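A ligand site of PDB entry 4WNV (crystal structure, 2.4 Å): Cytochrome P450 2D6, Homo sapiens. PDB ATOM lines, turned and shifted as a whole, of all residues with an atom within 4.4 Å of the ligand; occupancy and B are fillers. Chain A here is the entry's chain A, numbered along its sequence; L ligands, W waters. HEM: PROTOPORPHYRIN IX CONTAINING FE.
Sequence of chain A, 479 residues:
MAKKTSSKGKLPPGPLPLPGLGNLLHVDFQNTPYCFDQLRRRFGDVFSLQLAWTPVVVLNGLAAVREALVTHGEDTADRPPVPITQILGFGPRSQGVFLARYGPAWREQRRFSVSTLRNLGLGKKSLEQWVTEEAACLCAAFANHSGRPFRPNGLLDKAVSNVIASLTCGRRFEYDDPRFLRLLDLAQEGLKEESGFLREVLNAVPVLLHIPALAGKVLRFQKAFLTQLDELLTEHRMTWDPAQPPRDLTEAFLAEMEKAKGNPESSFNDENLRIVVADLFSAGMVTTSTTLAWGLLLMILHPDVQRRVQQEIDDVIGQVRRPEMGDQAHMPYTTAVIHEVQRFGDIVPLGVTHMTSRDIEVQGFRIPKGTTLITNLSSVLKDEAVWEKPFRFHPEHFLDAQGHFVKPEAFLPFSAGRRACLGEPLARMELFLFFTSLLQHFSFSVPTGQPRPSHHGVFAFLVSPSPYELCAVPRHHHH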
ATOM      1  N   LEU A  69     -36.333 -28.986  12.596  1.00  0.00           N
ATOM      2  CA  LEU A  69     -35.656 -27.957  13.387  1.00  0.00           C
ATOM      3  C   LEU A  69     -35.588 -26.583  12.692  1.00  0.00           C
ATOM      4  O   LEU A  69     -35.541 -25.571  13.353  1.00  0.00           O
ATOM      5  CB  LEU A  69     -34.260 -28.420  13.780  1.00  0.00           C
ATOM      6  CG  LEU A  69     -34.220 -29.647  14.699  1.00  0.00           C
ATOM      7  CD1 LEU A  69     -32.843 -29.848  15.319  1.00  0.00           C
ATOM      8  CD2 LEU A  69     -35.296 -29.584  15.794  1.00  0.00           C
ATOM      9  N   ARG A  79     -38.109 -28.035  25.078  1.00  0.00           N
ATOM     10  CA  ARG A  79     -37.537 -29.236  25.687  1.00  0.00           C
ATOM     11  C   ARG A  79     -38.613 -29.994  26.425  1.00  0.00           C
ATOM     12  O   ARG A  79     -39.591 -29.415  26.868  1.00  0.00           O
ATOM     13  CB  ARG A  79     -36.413 -28.881  26.678  1.00  0.00           C
ATOM     14  CG  ARG A  79     -35.293 -28.066  26.091  1.00  0.00           C
ATOM     15  CD  ARG A  79     -34.395 -28.928  25.237  1.00  0.00           C
ATOM     16  NE  ARG A  79     -33.152 -28.247  24.950  1.00  0.00           N
ATOM     17  CZ  ARG A  79     -32.435 -28.434  23.846  1.00  0.00           C
ATOM     18  NH1 ARG A  79     -31.316 -27.753  23.688  1.00  0.00           N
ATOM     19  NH2 ARG A  79     -32.836 -29.273  22.890  1.00  0.00           N
ATOM     20  N   VAL A  97     -30.224 -22.322  30.421  1.00  0.00           N
ATOM     21  CA  VAL A  97     -30.386 -22.277  28.974  1.00  0.00           C
ATOM     22  C   VAL A  97     -30.680 -23.667  28.428  1.00  0.00           C
ATOM     23  O   VAL A  97     -31.642 -23.857  27.698  1.00  0.00           O
ATOM     24  CB  VAL A  97     -29.123 -21.749  28.263  1.00  0.00           C
ATOM     25  CG1 VAL A  97     -29.262 -21.916  26.746  1.00  0.00           C
ATOM     26  CG2 VAL A  97     -28.866 -20.310  28.590  1.00  0.00           C
ATOM     27  N   PHE A  98     -29.836 -24.645  28.791  1.00  0.00           N
ATOM     28  CA  PHE A  98     -29.840 -25.960  28.146  1.00  0.00           C
ATOM     29  C   PHE A  98     -31.179 -26.667  28.221  1.00  0.00           C
ATOM     30  O   PHE A  98     -31.718 -27.079  27.200  1.00  0.00           O
ATOM     31  CB  PHE A  98     -28.756 -26.864  28.759  1.00  0.00           C
ATOM     32  CG  PHE A  98     -28.157 -27.857  27.772  1.00  0.00           C
ATOM     33  CD1 PHE A  98     -26.831 -27.769  27.409  1.00  0.00           C
ATOM     34  CD2 PHE A  98     -28.915 -28.860  27.213  1.00  0.00           C
ATOM     35  CE1 PHE A  98     -26.279 -28.652  26.509  1.00  0.00           C
ATOM     36  CE2 PHE A  98     -28.351 -29.769  26.320  1.00  0.00           C
ATOM     37  CZ  PHE A  98     -27.026 -29.655  25.972  1.00  0.00           C
ATOM     38  N   TRP A 106     -35.786 -18.779  28.550  1.00  0.00           N
ATOM     39  CA  TRP A 106     -34.763 -19.335  27.656  1.00  0.00           C
ATOM     40  C   TRP A 106     -34.182 -18.291  26.712  1.00  0.00           C
ATOM     41  O   TRP A 106     -32.968 -18.212  26.537  1.00  0.00           O
ATOM     42  CB  TRP A 106     -35.305 -20.501  26.799  1.00  0.00           C
ATOM     43  CG  TRP A 106     -34.385 -20.842  25.627  1.00  0.00           C
ATOM     44  CD1 TRP A 106     -33.256 -21.623  25.671  1.00  0.00           C
ATOM     45  CD2 TRP A 106     -34.492 -20.356  24.279  1.00  0.00           C
ATOM     46  NE1 TRP A 106     -32.666 -21.669  24.420  1.00  0.00           N
ATOM     47  CE2 TRP A 106     -33.400 -20.899  23.556  1.00  0.00           C
ATOM     48  CE3 TRP A 106     -35.398 -19.525  23.614  1.00  0.00           C
ATOM     49  CZ2 TRP A 106     -33.203 -20.647  22.194  1.00  0.00           C
ATOM     50  CZ3 TRP A 106     -35.197 -19.251  22.255  1.00  0.00           C
ATOM     51  CH2 TRP A 106     -34.108 -19.833  21.561  1.00  0.00           C
ATOM     52  N   ARG A 110     -30.383 -17.214  26.466  1.00  0.00           N
ATOM     53  CA  ARG A 110     -29.772 -17.619  25.206  1.00  0.00           C
ATOM     54  C   ARG A 110     -29.098 -16.422  24.534  1.00  0.00           C
ATOM     55  O   ARG A 110     -27.943 -16.514  24.101  1.00  0.00           O
ATOM     56  CB  ARG A 110     -30.815 -18.238  24.268  1.00  0.00           C
ATOM     57  CG  ARG A 110     -30.363 -18.437  22.822  1.00  0.00           C
ATOM     58  CD  ARG A 110     -29.621 -19.753  22.603  1.00  0.00           C
ATOM     59  NE  ARG A 110     -29.136 -19.860  21.223  1.00  0.00           N
ATOM     60  CZ  ARG A 110     -28.733 -20.983  20.635  1.00  0.00           C
ATOM     61  NH1 ARG A 110     -28.754 -22.134  21.306  1.00  0.00           N
ATOM     62  NH2 ARG A 110     -28.296 -20.973  19.387  1.00  0.00           N
ATOM     63  N   ILE A 164     -13.644 -22.788  30.005  1.00  0.00           N
ATOM     64  CA  ILE A 164     -14.947 -22.404  30.533  1.00  0.00           C
ATOM     65  C   ILE A 164     -14.788 -21.570  31.819  1.00  0.00           C
ATOM     66  O   ILE A 164     -15.497 -20.575  32.021  1.00  0.00           O
ATOM     67  CB  ILE A 164     -15.839 -23.620  30.839  1.00  0.00           C
ATOM     68  CG1 ILE A 164     -16.163 -24.398  29.576  1.00  0.00           C
ATOM     69  CG2 ILE A 164     -17.129 -23.160  31.519  1.00  0.00           C
ATOM     70  CD1 ILE A 164     -16.523 -23.505  28.370  1.00  0.00           C
ATOM     71  N   LEU A 167     -13.911 -18.103  30.650  1.00  0.00           N
ATOM     72  CA  LEU A 167     -15.133 -17.487  30.147  1.00  0.00           C
ATOM     73  C   LEU A 167     -16.037 -17.050  31.293  1.00  0.00           C
ATOM     74  O   LEU A 167     -16.543 -15.926  31.308  1.00  0.00           O
ATOM     75  CB  LEU A 167     -15.881 -18.475  29.232  1.00  0.00           C
ATOM     76  CG  LEU A 167     -17.394 -18.329  29.004  1.00  0.00           C
ATOM     77  CD1 LEU A 167     -17.695 -17.022  28.342  1.00  0.00           C
ATOM     78  CD2 LEU A 167     -17.960 -19.478  28.154  1.00  0.00           C
ATOM     79  N   LEU A 280     -23.017 -24.058  31.076  1.00  0.00           N
ATOM     80  CA  LEU A 280     -21.912 -23.820  30.143  1.00  0.00           C
ATOM     81  C   LEU A 280     -20.746 -24.816  30.374  1.00  0.00           C
ATOM     82  O   LEU A 280     -20.188 -25.355  29.410  1.00  0.00           O
ATOM     83  CB  LEU A 280     -21.436 -22.375  30.261  1.00  0.00           C
ATOM     84  CG  LEU A 280     -22.534 -21.379  29.873  1.00  0.00           C
ATOM     85  CD1 LEU A 280     -22.131 -19.965  30.183  1.00  0.00           C
ATOM     86  CD2 LEU A 280     -22.982 -21.527  28.387  1.00  0.00           C
ATOM     87  N   ALA A 283     -22.084 -28.339  29.287  1.00  0.00           N
ATOM     88  CA  ALA A 283     -22.214 -28.396  27.843  1.00  0.00           C
ATOM     89  C   ALA A 283     -20.868 -28.268  27.159  1.00  0.00           C
ATOM     90  O   ALA A 283     -20.651 -28.851  26.110  1.00  0.00           O
ATOM     91  CB  ALA A 283     -23.149 -27.283  27.369  1.00  0.00           C
ATOM     92  N   GLY A 284     -19.953 -27.510  27.769  1.00  0.00           N
ATOM     93  CA  GLY A 284     -18.685 -27.207  27.133  1.00  0.00           C
ATOM     94  C   GLY A 284     -17.485 -28.064  27.488  1.00  0.00           C
ATOM     95  O   GLY A 284     -16.474 -28.040  26.784  1.00  0.00           O
ATOM     96  N   THR A 287     -17.843 -32.404  25.912  1.00  0.00           N
ATOM     97  CA  THR A 287     -17.903 -32.367  24.451  1.00  0.00           C
ATOM     98  C   THR A 287     -16.539 -32.020  23.831  1.00  0.00           C
ATOM     99  O   THR A 287     -15.954 -32.829  23.110  1.00  0.00           O
ATOM    100  CB  THR A 287     -18.948 -31.355  23.959  1.00  0.00           C
ATOM    101  OG1 THR A 287     -18.730 -30.101  24.617  1.00  0.00           O
ATOM    102  CG2 THR A 287     -20.387 -31.841  24.261  1.00  0.00           C
ATOM    103  N   THR A 288     -16.020 -30.833  24.130  1.00  0.00           N
ATOM    104  CA  THR A 288     -14.766 -30.421  23.523  1.00  0.00           C
ATOM    105  C   THR A 288     -13.618 -31.376  23.904  1.00  0.00           C
ATOM    106  O   THR A 288     -12.734 -31.642  23.110  1.00  0.00           O
ATOM    107  CB  THR A 288     -14.389 -29.001  23.942  1.00  0.00           C
ATOM    108  OG1 THR A 288     -15.529 -28.148  23.767  1.00  0.00           O
ATOM    109  CG2 THR A 288     -13.266 -28.489  23.076  1.00  0.00           C
ATOM    110  N   THR A 291     -14.057 -34.811  22.069  1.00  0.00           N
ATOM    111  CA  THR A 291     -13.689 -34.574  20.673  1.00  0.00           C
ATOM    112  C   THR A 291     -12.161 -34.538  20.511  1.00  0.00           C
ATOM    113  O   THR A 291     -11.622 -35.174  19.597  1.00  0.00           O
ATOM    114  CB  THR A 291     -14.282 -33.270  20.124  1.00  0.00           C
ATOM    115  OG1 THR A 291     -15.710 -33.343  20.200  1.00  0.00           O
ATOM    116  CG2 THR A 291     -13.876 -33.057  18.673  1.00  0.00           C
ATOM    117  N   GLN A 342     -14.586 -34.564  14.166  1.00  0.00           N
ATOM    118  CA  GLN A 342     -15.938 -34.376  14.691  1.00  0.00           C
ATOM    119  C   GLN A 342     -16.962 -35.289  14.018  1.00  0.00           C
ATOM    120  O   GLN A 342     -17.827 -35.846  14.688  1.00  0.00           O
ATOM    121  CB  GLN A 342     -16.388 -32.932  14.527  1.00  0.00           C
ATOM    122  CG  GLN A 342     -15.597 -31.917  15.339  1.00  0.00           C
ATOM    123  CD  GLN A 342     -16.339 -30.593  15.397  1.00  0.00           C
ATOM    124  OE1 GLN A 342     -16.080 -29.696  14.595  1.00  0.00           O
ATOM    125  NE2 GLN A 342     -17.316 -30.486  16.302  1.00  0.00           N
ATOM    126  N   ILE A 347     -19.836 -37.515  18.610  1.00  0.00           N
ATOM    127  CA  ILE A 347     -19.819 -37.698  20.061  1.00  0.00           C
ATOM    128  C   ILE A 347     -21.171 -37.510  20.709  1.00  0.00           C
ATOM    129  O   ILE A 347     -21.338 -37.886  21.865  1.00  0.00           O
ATOM    130  CB  ILE A 347     -18.821 -36.715  20.728  1.00  0.00           C
ATOM    131  CG1 ILE A 347     -19.265 -35.275  20.552  1.00  0.00           C
ATOM    132  CG2 ILE A 347     -17.455 -36.872  20.150  1.00  0.00           C
ATOM    133  CD1 ILE A 347     -18.625 -34.328  21.571  1.00  0.00           C
ATOM    134  N   VAL A 348     -22.123 -36.902  19.986  1.00  0.00           N
ATOM    135  CA  VAL A 348     -23.494 -36.758  20.484  1.00  0.00           C
ATOM    136  C   VAL A 348     -24.492 -37.339  19.464  1.00  0.00           C
ATOM    137  O   VAL A 348     -25.281 -36.595  18.847  1.00  0.00           O
ATOM    138  CB  VAL A 348     -23.865 -35.279  20.787  1.00  0.00           C
ATOM    139  CG1 VAL A 348     -25.024 -35.241  21.750  1.00  0.00           C
ATOM    140  CG2 VAL A 348     -22.687 -34.543  21.425  1.00  0.00           C
ATOM    141  N   GLY A 351     -28.059 -36.412  19.780  1.00  0.00           N
ATOM    142  CA  GLY A 351     -28.220 -35.024  20.210  1.00  0.00           C
ATOM    143  C   GLY A 351     -28.882 -34.826  21.569  1.00  0.00           C
ATOM    144  O   GLY A 351     -28.669 -35.596  22.492  1.00  0.00           O
ATOM    145  N   VAL A 352     -29.704 -33.780  21.664  1.00  0.00           N
ATOM    146  CA  VAL A 352     -30.467 -33.501  22.886  1.00  0.00           C
ATOM    147  C   VAL A 352     -31.939 -33.414  22.500  1.00  0.00           C
ATOM    148  O   VAL A 352     -32.283 -32.845  21.470  1.00  0.00           O
ATOM    149  CB  VAL A 352     -30.001 -32.207  23.543  1.00  0.00           C
ATOM    150  CG1 VAL A 352     -30.712 -31.985  24.894  1.00  0.00           C
ATOM    151  CG2 VAL A 352     -28.477 -32.244  23.721  1.00  0.00           C
ATOM    152  N   HIS A 354     -35.769 -32.622  21.807  1.00  0.00           N
ATOM    153  CA  HIS A 354     -36.635 -31.467  21.659  1.00  0.00           C
ATOM    154  C   HIS A 354     -38.044 -31.937  21.978  1.00  0.00           C
ATOM    155  O   HIS A 354     -38.283 -33.156  22.060  1.00  0.00           O
ATOM    156  CB  HIS A 354     -36.564 -30.889  20.249  1.00  0.00           C
ATOM    157  CG  HIS A 354     -35.246 -30.293  19.897  1.00  0.00           C
ATOM    158  ND1 HIS A 354     -35.099 -28.979  19.487  1.00  0.00           N
ATOM    159  CD2 HIS A 354     -33.999 -30.829  19.886  1.00  0.00           C
ATOM    160  CE1 HIS A 354     -33.822 -28.739  19.234  1.00  0.00           C
ATOM    161  NE2 HIS A 354     -33.133 -29.847  19.461  1.00  0.00           N
ATOM    162  N   LEU A 377     -28.492 -37.185  14.996  1.00  0.00           N
ATOM    163  CA  LEU A 377     -27.355 -36.532  14.351  1.00  0.00           C
ATOM    164  C   LEU A 377     -26.366 -37.509  13.717  1.00  0.00           C
ATOM    165  O   LEU A 377     -25.871 -37.255  12.618  1.00  0.00           O
ATOM    166  CB  LEU A 377     -26.606 -35.661  15.376  1.00  0.00           C
ATOM    167  CG  LEU A 377     -27.392 -34.524  16.036  1.00  0.00           C
ATOM    168  CD1 LEU A 377     -26.477 -33.626  16.868  1.00  0.00           C
ATOM    169  CD2 LEU A 377     -28.123 -33.688  14.992  1.00  0.00           C
ATOM    170  N   PRO A 413     -22.622 -31.502  13.577  1.00  0.00           N
ATOM    171  CA  PRO A 413     -22.395 -32.073  14.907  1.00  0.00           C
ATOM    172  C   PRO A 413     -22.950 -31.172  16.023  1.00  0.00           C
ATOM    173  O   PRO A 413     -23.030 -31.613  17.163  1.00  0.00           O
ATOM    174  CB  PRO A 413     -20.889 -32.163  14.970  1.00  0.00           C
ATOM    175  CG  PRO A 413     -20.440 -30.951  14.182  1.00  0.00           C
ATOM    176  CD  PRO A 413     -21.387 -30.922  13.016  1.00  0.00           C
ATOM    177  N   PHE A 414     -23.357 -29.950  15.687  1.00  0.00           N
ATOM    178  CA  PHE A 414     -23.896 -29.010  16.673  1.00  0.00           C
ATOM    179  C   PHE A 414     -25.412 -28.892  16.578  1.00  0.00           C
ATOM    180  O   PHE A 414     -25.996 -27.992  17.175  1.00  0.00           O
ATOM    181  CB  PHE A 414     -23.261 -27.629  16.512  1.00  0.00           C
ATOM    182  CG  PHE A 414     -21.755 -27.607  16.643  1.00  0.00           C
ATOM    183  CD1 PHE A 414     -20.945 -27.543  15.510  1.00  0.00           C
ATOM    184  CD2 PHE A 414     -21.151 -27.627  17.893  1.00  0.00           C
ATOM    185  CE1 PHE A 414     -19.554 -27.498  15.626  1.00  0.00           C
ATOM    186  CE2 PHE A 414     -19.743 -27.595  18.013  1.00  0.00           C
ATOM    187  CZ  PHE A 414     -18.955 -27.530  16.878  1.00  0.00           C
ATOM    188  N   SER A 415     -26.045 -29.792  15.828  1.00  0.00           N
ATOM    189  CA  SER A 415     -27.493 -29.739  15.509  1.00  0.00           C
ATOM    190  C   SER A 415     -27.845 -28.513  14.676  1.00  0.00           C
ATOM    191  O   SER A 415     -26.983 -27.988  13.959  1.00  0.00           O
ATOM    192  CB  SER A 415     -28.347 -29.784  16.786  1.00  0.00           C
ATOM    193  OG  SER A 415     -29.724 -29.847  16.477  1.00  0.00           O
ATOM    194  N   ARG A 419     -32.126 -24.041  18.863  1.00  0.00           N
ATOM    195  CA  ARG A 419     -31.434 -24.641  19.993  1.00  0.00           C
ATOM    196  C   ARG A 419     -30.037 -25.175  19.666  1.00  0.00           C
ATOM    197  O   ARG A 419     -29.339 -25.662  20.551  1.00  0.00           O
ATOM    198  CB  ARG A 419     -32.267 -25.770  20.562  1.00  0.00           C
ATOM    199  CG  ARG A 419     -33.522 -25.280  21.216  1.00  0.00           C
ATOM    200  CD  ARG A 419     -33.166 -24.668  22.555  1.00  0.00           C
ATOM    201  NE  ARG A 419     -34.395 -24.506  23.266  1.00  0.00           N
ATOM    202  CZ  ARG A 419     -34.567 -24.664  24.564  1.00  0.00           C
ATOM    203  NH1 ARG A 419     -33.536 -24.949  25.375  1.00  0.00           N
ATOM    204  NH2 ARG A 419     -35.809 -24.487  25.039  1.00  0.00           N
ATOM    205  N   ALA A 420     -29.640 -25.069  18.406  1.00  0.00           N
ATOM    206  CA  ALA A 420     -28.314 -25.534  17.985  1.00  0.00           C
ATOM    207  C   ALA A 420     -27.230 -24.982  18.926  1.00  0.00           C
ATOM    208  O   ALA A 420     -27.389 -23.887  19.471  1.00  0.00           O
ATOM    209  CB  ALA A 420     -28.037 -25.124  16.556  1.00  0.00           C
ATOM    210  N   CYS A 421     -26.172 -25.766  19.151  1.00  0.00           N
ATOM    211  CA  CYS A 421     -25.153 -25.433  20.148  1.00  0.00           C
ATOM    212  C   CYS A 421     -24.799 -23.934  20.153  1.00  0.00           C
ATOM    213  O   CYS A 421     -24.379 -23.402  19.140  1.00  0.00           O
ATOM    214  CB  CYS A 421     -23.901 -26.271  19.875  1.00  0.00           C
ATOM    215  SG  CYS A 421     -22.545 -26.060  21.115  1.00  0.00           S
ATOM    216  N   LEU A 422     -25.008 -23.242  21.276  1.00  0.00           N
ATOM    217  CA  LEU A 422     -24.599 -21.835  21.309  1.00  0.00           C
ATOM    218  C   LEU A 422     -23.076 -21.726  21.450  1.00  0.00           C
ATOM    219  O   LEU A 422     -22.504 -20.674  21.194  1.00  0.00           O
ATOM    220  CB  LEU A 422     -25.307 -21.061  22.429  1.00  0.00           C
ATOM    221  CG  LEU A 422     -25.179 -21.335  23.934  1.00  0.00           C
ATOM    222  CD1 LEU A 422     -23.847 -20.829  24.575  1.00  0.00           C
ATOM    223  CD2 LEU A 422     -26.383 -20.693  24.608  1.00  0.00           C
ATOM    224  N   GLY A 423     -22.426 -22.838  21.783  1.00  0.00           N
ATOM    225  CA  GLY A 423     -21.004 -22.821  22.056  1.00  0.00           C
ATOM    226  C   GLY A 423     -20.142 -23.036  20.835  1.00  0.00           C
ATOM    227  O   GLY A 423     -18.918 -23.011  20.924  1.00  0.00           O
ATOM    228  N   LEU A 426     -16.934 -20.964  20.145  1.00  0.00           N
ATOM    229  CA  LEU A 426     -15.876 -21.253  21.111  1.00  0.00           C
ATOM    230  C   LEU A 426     -15.271 -22.637  20.874  1.00  0.00           C
ATOM    231  O   LEU A 426     -14.064 -22.820  20.923  1.00  0.00           O
ATOM    232  CB  LEU A 426     -16.403 -21.144  22.544  1.00  0.00           C
ATOM    233  CG  LEU A 426     -15.391 -21.404  23.660  1.00  0.00           C
ATOM    234  CD1 LEU A 426     -14.148 -20.529  23.477  1.00  0.00           C
ATOM    235  CD2 LEU A 426     -16.018 -21.149  25.024  1.00  0.00           C
ATOM    236  N   ALA A 427     -16.139 -23.610  20.598  1.00  0.00           N
ATOM    237  CA  ALA A 427     -15.690 -24.976  20.352  1.00  0.00           C
ATOM    238  C   ALA A 427     -14.738 -25.042  19.164  1.00  0.00           C
ATOM    239  O   ALA A 427     -13.758 -25.763  19.203  1.00  0.00           O
ATOM    240  CB  ALA A 427     -16.863 -25.889  20.136  1.00  0.00           C
ATOM    241  N   GLU A 430     -11.431 -23.644  20.282  1.00  0.00           N
ATOM    242  CA  GLU A 430     -10.695 -24.578  21.133  1.00  0.00           C
ATOM    243  C   GLU A 430     -10.125 -25.749  20.320  1.00  0.00           C
ATOM    244  O   GLU A 430      -8.965 -26.135  20.502  1.00  0.00           O
ATOM    245  CB  GLU A 430     -11.576 -25.125  22.238  1.00  0.00           C
ATOM    246  CG  GLU A 430     -12.041 -24.104  23.273  1.00  0.00           C
ATOM    247  CD  GLU A 430     -12.747 -24.790  24.424  1.00  0.00           C
ATOM    248  OE1 GLU A 430     -12.070 -25.489  25.193  1.00  0.00           O
ATOM    249  OE2 GLU A 430     -13.994 -24.695  24.528  1.00  0.00           O
HETATM  250  CHA HEM L   1     -26.335 -27.456  22.849  1.00  0.00           C
HETATM  251  CHB HEM L   1     -22.951 -30.217  20.693  1.00  0.00           C
HETATM  252  CHC HEM L   1     -19.552 -27.419  22.810  1.00  0.00           C
HETATM  253  CHD HEM L   1     -22.925 -24.820  25.097  1.00  0.00           C
HETATM  254  C1A HEM L   1     -25.751 -28.467  22.101  1.00  0.00           C
HETATM  255  C2A HEM L   1     -26.439 -29.488  21.335  1.00  0.00           C
HETATM  256  C3A HEM L   1     -25.524 -30.241  20.741  1.00  0.00           C
HETATM  257  C4A HEM L   1     -24.198 -29.724  21.092  1.00  0.00           C
HETATM  258  CMA HEM L   1     -25.847 -31.428  19.866  1.00  0.00           C
HETATM  259  CAA HEM L   1     -27.959 -29.704  21.243  1.00  0.00           C
HETATM  260  CBA HEM L   1     -28.638 -28.844  20.182  1.00  0.00           C
HETATM  261  CGA HEM L   1     -30.110 -29.203  20.149  1.00  0.00           C
HETATM  262  O1A HEM L   1     -30.783 -29.174  21.232  1.00  0.00           O
HETATM  263  O2A HEM L   1     -30.629 -29.517  19.036  1.00  0.00           O
HETATM  264  C1B HEM L   1     -21.702 -29.682  21.041  1.00  0.00           C
HETATM  265  C2B HEM L   1     -20.389 -30.094  20.545  1.00  0.00           C
HETATM  266  C3B HEM L   1     -19.458 -29.315  21.138  1.00  0.00           C
HETATM  267  C4B HEM L   1     -20.152 -28.384  22.017  1.00  0.00           C
HETATM  268  CMB HEM L   1     -20.172 -31.201  19.552  1.00  0.00           C
HETATM  269  CAB HEM L   1     -17.914 -29.292  21.022  1.00  0.00           C
HETATM  270  CBB HEM L   1     -17.176 -30.148  20.302  1.00  0.00           C
HETATM  271  C1C HEM L   1     -20.145 -26.451  23.593  1.00  0.00           C
HETATM  272  C2C HEM L   1     -19.479 -25.367  24.284  1.00  0.00           C
HETATM  273  C3C HEM L   1     -20.411 -24.645  24.932  1.00  0.00           C
HETATM  274  C4C HEM L   1     -21.688 -25.259  24.639  1.00  0.00           C
HETATM  275  CMC HEM L   1     -17.982 -25.134  24.260  1.00  0.00           C
HETATM  276  CAC HEM L   1     -20.292 -23.388  25.821  1.00  0.00           C
HETATM  277  CBC HEM L   1     -19.298 -22.507  25.802  1.00  0.00           C
HETATM  278  C1D HEM L   1     -24.153 -25.330  24.724  1.00  0.00           C
HETATM  279  C2D HEM L   1     -25.445 -24.928  25.242  1.00  0.00           C
HETATM  280  C3D HEM L   1     -26.376 -25.662  24.609  1.00  0.00           C
HETATM  281  C4D HEM L   1     -25.721 -26.542  23.675  1.00  0.00           C
HETATM  282  CMD HEM L   1     -25.685 -23.867  26.315  1.00  0.00           C
HETATM  283  CAD HEM L   1     -27.902 -25.558  24.829  1.00  0.00           C
HETATM  284  CBD HEM L   1     -28.419 -24.582  23.765  1.00  0.00           C
HETATM  285  CGD HEM L   1     -29.910 -24.376  23.908  1.00  0.00           C
HETATM  286  O1D HEM L   1     -30.407 -23.294  23.545  1.00  0.00           O
HETATM  287  O2D HEM L   1     -30.606 -25.290  24.417  1.00  0.00           O
HETATM  288  NA  HEM L   1     -24.394 -28.619  21.906  1.00  0.00           N
HETATM  289  NB  HEM L   1     -21.502 -28.652  21.937  1.00  0.00           N
HETATM  290  NC  HEM L   1     -21.494 -26.346  23.835  1.00  0.00           N
HETATM  291  ND  HEM L   1     -24.360 -26.321  23.778  1.00  0.00           N
HETATM  292 FE   HEM L   1     -22.906 -27.392  22.753  1.00  0.00          FE
HETATM  293  O   HOH W   1     -23.181 -28.912  24.286  1.00  0.00           O
HETATM  294  O   HOH W   2     -24.214 -31.274  23.850  1.00  0.00           O
HETATM  295  O   HOH W   3     -29.798 -32.420  19.112  1.00  0.00           O
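SG of Cys 421 binds FE of the ligand, 2.1 Å away.
NE2 of His 354 lies within hydrogen-bond range of O2A of the ligand (2.6 Å).
The guanidinium group (NH2) of Arg 79 is in salt-bridge range of an oxygen (O1A) of the ligand, at 2.6 Å.
OG of Ser 415 sits at hydrogen-bond distance from O2A of the ligand (2.7 Å).
An oxygen (O1D) of the ligand lies within hydrogen-bond range of the indole nitrogen of Trp 106, at 2.9 Å.
The guanidinium group of Arg 110 is in salt-bridge range of an oxygen (O1D) of the ligand (3.0 Å).
The guanidinium group (NH1) of Arg 419 is in salt-bridge range of an oxygen (O2D) of the ligand.
The backbone carbonyl oxygen (O) of Phe 98 lies close to an oxygen (O2D) of the ligand.
A nitrogen (NC) of the ligand sits close to the backbone carbonyl oxygen (O) of Ala 283 (3.5 Å).
Val 97 touches the ligand.
Ile 164 touches the ligand (CD1 to CBC, 3.9 Å).
CA of Gly 284 touches C2C of the ligand (3.5 Å).
Thr 287 touches the ligand.
OG1 of Thr 288 touches CAB of the ligand, at 3.8 Å.
OG1 of Thr 291 touches CBB of the ligand (3.5 Å).
Val 352 touches the ligand.
Leu 377 touches the ligand.
Pro 413 touches the ligand.
Phe 414 touches the ligand.
Ala 420 touches the ligand.
CG of Leu 422 touches CMD of the ligand, at 3.5 Å.
Gly 423 touches the ligand (CA to C3C, 3.5 Å).
Leu 426 touches the ligand.
CB of Ala 427 touches CAB of the ligand (3.7 Å).
Hydrophobic or aromatic side chains within 4 Å of the ligand: Val 97, Phe 98, Trp 106, Ile 164, Ala 283, Val 352, His 354, Leu 377, Phe 414, Leu 422, Leu 426 and Ala 427.
The nearest printed residue that does not touch the ligand is Gln 342 (4.02 Å).
The backbone NH of Gly 423 lies close to the side-chain sulfur of Cys 421 (3.3 Å).
The backbone NH (N) of Cys 421 is in hydrogen-bond range of the backbone carbonyl oxygen (O) of Phe 414.
NH2 of Arg 79 sits at hydrogen-bond distance from NE2 of His 354 (3.5 Å).
The guanidinium group (NE) of Arg 79 sits at hydrogen-bond distance from the backbone carbonyl oxygen (O) of Phe 98 (2.9 Å).
The guanidinium group of Arg 110 is in hydrogen-bond range of the backbone carbonyl oxygen of Ala 420 (2.9 Å).
O of Val 97 is in hydrogen-bond range of NH1 of Arg 419 (3.2 Å).
The backbone carbonyl oxygen (O) of Thr 287 sits at hydrogen-bond distance from the side-chain hydroxyl (OG1) of Thr 291.
O of Gly 284 sits at hydrogen-bond distance from OG1 of Thr 288 (3.2 Å).
Water W3 bridges N of Val 352 and O2A of the ligand.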
